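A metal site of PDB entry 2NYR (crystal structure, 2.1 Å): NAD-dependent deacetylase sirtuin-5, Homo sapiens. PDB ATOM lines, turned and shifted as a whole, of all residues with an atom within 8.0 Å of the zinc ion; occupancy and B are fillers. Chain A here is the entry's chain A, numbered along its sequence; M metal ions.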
ATOM      1  N   ARG A 134      10.778 -34.831  21.512  1.00  0.00           N
ATOM      2  CA  ARG A 134      11.591 -33.675  21.118  1.00  0.00           C
ATOM      3  C   ARG A 134      10.832 -32.839  20.089  1.00  0.00           C
ATOM      4  O   ARG A 134      10.280 -33.368  19.132  1.00  0.00           O
ATOM      5  CB  ARG A 134      12.956 -34.107  20.563  1.00  0.00           C
ATOM      6  CG  ARG A 134      13.882 -32.922  20.249  1.00  0.00           C
ATOM      7  CD  ARG A 134      15.352 -33.297  20.245  1.00  0.00           C
ATOM      8  NE  ARG A 134      15.782 -33.875  18.975  1.00  0.00           N
ATOM      9  CZ  ARG A 134      15.977 -35.172  18.764  1.00  0.00           C
ATOM     10  NH1 ARG A 134      15.754 -36.053  19.723  1.00  0.00           N
ATOM     11  NH2 ARG A 134      16.388 -35.588  17.571  1.00  0.00           N
ATOM     12  N   CYS A 135      10.835 -31.527  20.288  1.00  0.00           N
ATOM     13  CA  CYS A 135      10.198 -30.632  19.355  1.00  0.00           C
ATOM     14  C   CYS A 135      11.120 -30.316  18.181  1.00  0.00           C
ATOM     15  O   CYS A 135      12.233 -29.832  18.379  1.00  0.00           O
ATOM     16  CB  CYS A 135       9.778 -29.347  20.066  1.00  0.00           C
ATOM     17  SG  CYS A 135       8.990 -28.184  18.965  1.00  0.00           S
ATOM     18  N   THR A 136      10.638 -30.586  16.970  1.00  0.00           N
ATOM     19  CA  THR A 136      11.408 -30.355  15.737  1.00  0.00           C
ATOM     20  C   THR A 136      11.544 -28.874  15.375  1.00  0.00           C
ATOM     21  O   THR A 136      12.288 -28.514  14.452  1.00  0.00           O
ATOM     22  CB  THR A 136      10.790 -31.144  14.548  1.00  0.00           C
ATOM     23  OG1 THR A 136       9.446 -30.704  14.324  1.00  0.00           O
ATOM     24  CG2 THR A 136      10.800 -32.643  14.830  1.00  0.00           C
ATOM     25  N   SER A 137      10.829 -28.018  16.110  1.00  0.00           N
ATOM     26  CA  SER A 137      10.916 -26.574  15.917  1.00  0.00           C
ATOM     27  C   SER A 137      11.828 -25.888  16.946  1.00  0.00           C
ATOM     28  O   SER A 137      12.795 -25.221  16.582  1.00  0.00           O
ATOM     29  CB  SER A 137       9.523 -25.947  15.928  1.00  0.00           C
ATOM     30  OG  SER A 137       8.865 -26.173  14.706  1.00  0.00           O
ATOM     31  N   CYS A 138      11.505 -26.065  18.226  1.00  0.00           N
ATOM     32  CA  CYS A 138      12.205 -25.347  19.290  1.00  0.00           C
ATOM     33  C   CYS A 138      13.314 -26.175  19.953  1.00  0.00           C
ATOM     34  O   CYS A 138      14.206 -25.623  20.611  1.00  0.00           O
ATOM     35  CB  CYS A 138      11.226 -24.796  20.336  1.00  0.00           C
ATOM     36  SG  CYS A 138      10.538 -26.047  21.459  1.00  0.00           S
ATOM     37  N   GLY A 139      13.242 -27.494  19.795  1.00  0.00           N
ATOM     38  CA  GLY A 139      14.273 -28.381  20.302  1.00  0.00           C
ATOM     39  C   GLY A 139      14.093 -28.808  21.746  1.00  0.00           C
ATOM     40  O   GLY A 139      14.958 -29.480  22.307  1.00  0.00           O
ATOM     41  N   VAL A 140      12.966 -28.425  22.354  1.00  0.00           N
ATOM     42  CA  VAL A 140      12.716 -28.761  23.750  1.00  0.00           C
ATOM     43  C   VAL A 140      12.422 -30.259  23.918  1.00  0.00           C
ATOM     44  O   VAL A 140      11.602 -30.839  23.213  1.00  0.00           O
ATOM     45  CB  VAL A 140      11.589 -27.889  24.356  1.00  0.00           C
ATOM     46  CG1 VAL A 140      11.082 -28.466  25.673  1.00  0.00           C
ATOM     47  CG2 VAL A 140      12.084 -26.461  24.557  1.00  0.00           C
ATOM     48  N   VAL A 141      13.134 -30.880  24.859  1.00  0.00           N
ATOM     49  CA  VAL A 141      12.899 -32.282  25.215  1.00  0.00           C
ATOM     50  C   VAL A 141      11.973 -32.326  26.429  1.00  0.00           C
ATOM     51  O   VAL A 141      12.272 -31.715  27.461  1.00  0.00           O
ATOM     52  CB  VAL A 141      14.216 -33.040  25.478  1.00  0.00           C
ATOM     53  CG1 VAL A 141      13.938 -34.503  25.847  1.00  0.00           C
ATOM     54  CG2 VAL A 141      15.138 -32.939  24.272  1.00  0.00           C
ATOM     55  N   ARG A 175       1.892 -32.056  19.140  1.00  0.00           N
ATOM     56  CA  ARG A 175       2.478 -30.731  18.954  1.00  0.00           C
ATOM     57  C   ARG A 175       3.105 -30.212  20.250  1.00  0.00           C
ATOM     58  O   ARG A 175       2.702 -30.592  21.356  1.00  0.00           O
ATOM     59  CB  ARG A 175       1.435 -29.730  18.425  1.00  0.00           C
ATOM     60  CG  ARG A 175       0.601 -30.186  17.225  1.00  0.00           C
ATOM     61  CD  ARG A 175       1.413 -30.494  15.953  1.00  0.00           C
ATOM     62  NE  ARG A 175       2.195 -29.363  15.486  1.00  0.00           N
ATOM     63  CZ  ARG A 175       2.528 -29.157  14.209  1.00  0.00           C
ATOM     64  NH1 ARG A 175       2.142 -29.997  13.258  1.00  0.00           N
ATOM     65  NH2 ARG A 175       3.261 -28.093  13.888  1.00  0.00           N
ATOM     66  N   CYS A 176       4.099 -29.333  20.093  1.00  0.00           N
ATOM     67  CA  CYS A 176       4.759 -28.744  21.239  1.00  0.00           C
ATOM     68  C   CYS A 176       3.792 -27.851  21.979  1.00  0.00           C
ATOM     69  O   CYS A 176       2.984 -27.159  21.365  1.00  0.00           O
ATOM     70  CB  CYS A 176       5.959 -27.925  20.778  1.00  0.00           C
ATOM     71  SG  CYS A 176       7.005 -27.289  22.115  1.00  0.00           S
ATOM     72  N   GLU A 177       3.854 -27.888  23.310  1.00  0.00           N
ATOM     73  CA  GLU A 177       2.971 -27.074  24.150  1.00  0.00           C
ATOM     74  C   GLU A 177       3.722 -25.934  24.817  1.00  0.00           C
ATOM     75  O   GLU A 177       3.167 -25.261  25.689  1.00  0.00           O
ATOM     76  CB  GLU A 177       2.205 -27.954  25.152  1.00  0.00           C
ATOM     77  CG  GLU A 177       1.074 -28.744  24.468  1.00  0.00           C
ATOM     78  CD  GLU A 177       0.434 -29.824  25.340  1.00  0.00           C
ATOM     79  OE1 GLU A 177       0.111 -29.546  26.514  1.00  0.00           O
ATOM     80  OE2 GLU A 177       0.218 -30.945  24.816  1.00  0.00           O
ATOM     81  N   GLU A 178       4.971 -25.702  24.412  1.00  0.00           N
ATOM     82  CA  GLU A 178       5.675 -24.469  24.821  1.00  0.00           C
ATOM     83  C   GLU A 178       4.909 -23.283  24.241  1.00  0.00           C
ATOM     84  O   GLU A 178       4.492 -23.315  23.083  1.00  0.00           O
ATOM     85  CB  GLU A 178       7.130 -24.451  24.348  1.00  0.00           C
ATOM     86  CG  GLU A 178       8.044 -25.563  24.886  1.00  0.00           C
ATOM     87  CD  GLU A 178       8.400 -25.415  26.360  1.00  0.00           C
ATOM     88  OE1 GLU A 178       8.944 -24.358  26.758  1.00  0.00           O
ATOM     89  OE2 GLU A 178       8.154 -26.367  27.118  1.00  0.00           O
ATOM     90  N   ALA A 179       4.716 -22.232  25.046  1.00  0.00           N
ATOM     91  CA  ALA A 179       3.939 -21.066  24.638  1.00  0.00           C
ATOM     92  C   ALA A 179       4.506 -20.410  23.380  1.00  0.00           C
ATOM     93  O   ALA A 179       5.669 -20.013  23.335  1.00  0.00           O
ATOM     94  CB  ALA A 179       3.841 -20.053  25.772  1.00  0.00           C
ATOM     95  N   GLY A 180       3.673 -20.337  22.345  1.00  0.00           N
ATOM     96  CA  GLY A 180       4.060 -19.729  21.080  1.00  0.00           C
ATOM     97  C   GLY A 180       4.844 -20.599  20.125  1.00  0.00           C
ATOM     98  O   GLY A 180       5.235 -20.146  19.052  1.00  0.00           O
ATOM     99  N   CYS A 181       5.101 -21.850  20.489  1.00  0.00           N
ATOM    100  CA  CYS A 181       5.785 -22.762  19.577  1.00  0.00           C
ATOM    101  C   CYS A 181       4.819 -23.519  18.658  1.00  0.00           C
ATOM    102  O   CYS A 181       4.596 -23.095  17.519  1.00  0.00           O
ATOM    103  CB  CYS A 181       6.693 -23.743  20.327  1.00  0.00           C
ATOM    104  SG  CYS A 181       7.639 -24.784  19.212  1.00  0.00           S
ATOM    105  N   GLY A 182       4.252 -24.614  19.156  1.00  0.00           N
ATOM    106  CA  GLY A 182       3.274 -25.403  18.404  1.00  0.00           C
ATOM    107  C   GLY A 182       3.902 -26.306  17.347  1.00  0.00           C
ATOM    108  O   GLY A 182       3.217 -26.777  16.435  1.00  0.00           O
ATOM    109  N   GLY A 183       5.208 -26.536  17.494  1.00  0.00           N
ATOM    110  CA  GLY A 183       5.965 -27.347  16.550  1.00  0.00           C
ATOM    111  C   GLY A 183       5.596 -28.816  16.587  1.00  0.00           C
ATOM    112  O   GLY A 183       4.965 -29.288  17.541  1.00  0.00           O
ATOM    113  N   LEU A 184       5.998 -29.539  15.552  1.00  0.00           N
ATOM    114  CA  LEU A 184       5.725 -30.959  15.463  1.00  0.00           C
ATOM    115  C   LEU A 184       6.674 -31.730  16.355  1.00  0.00           C
ATOM    116  O   LEU A 184       7.897 -31.547  16.304  1.00  0.00           O
ATOM    117  CB  LEU A 184       5.822 -31.432  14.020  1.00  0.00           C
ATOM    118  CG  LEU A 184       5.732 -32.935  13.769  1.00  0.00           C
ATOM    119  CD1 LEU A 184       4.329 -33.456  14.050  1.00  0.00           C
ATOM    120  CD2 LEU A 184       6.122 -33.217  12.342  1.00  0.00           C
ATOM    121  N   LEU A 185       6.118 -32.599  17.201  1.00  0.00           N
ATOM    122  CA  LEU A 185       6.943 -33.419  18.075  1.00  0.00           C
ATOM    123  C   LEU A 185       7.377 -34.703  17.381  1.00  0.00           C
ATOM    124  O   LEU A 185       6.679 -35.240  16.533  1.00  0.00           O
ATOM    125  CB  LEU A 185       6.223 -33.723  19.401  1.00  0.00           C
ATOM    126  CG  LEU A 185       5.768 -32.541  20.270  1.00  0.00           C
ATOM    127  CD1 LEU A 185       4.993 -33.028  21.489  1.00  0.00           C
ATOM    128  CD2 LEU A 185       6.924 -31.646  20.705  1.00  0.00           C
HETATM  129 ZN    ZN M   1       8.537 -26.470  20.521  1.00  0.00          ZN
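The backbone NH (N) of Val 140 lies close to the side-chain sulfur (SG) of Cys 138 (3.5 Å).
SG of Cys 181 lies close to N of Gly 183, at 3.5 Å.
The side-chain sulfur of Cys 176 lies close to the backbone NH of Glu 178 (3.5 Å).
O of Gly 183 sits at hydrogen-bond distance from N of Cys 176, at 2.7 Å.
The side-chain sulfur (SG) of Cys 135 sits close to the backbone NH (N) of Ser 137 (3.4 Å).
N of Cys 135 is in hydrogen-bond range of O of Val 140.
Four residues have an atom within 4 Å of the zinc ion: Cys 135, Cys 138, Cys 176 and Cys 181.
Along chain A the residues within 4 Å of the zinc ion span positions 135 to 181.
The zinc ion is bound by the side-chain sulfur of Cys 138 (2.3 Å), the side-chain sulfur of Cys 181 (2.3 Å), the side-chain sulfur of Cys 176 (2.4 Å) and the side-chain sulfur of Cys 135 (2.4 Å).
The zinc ion has four donor atoms within binding distance.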
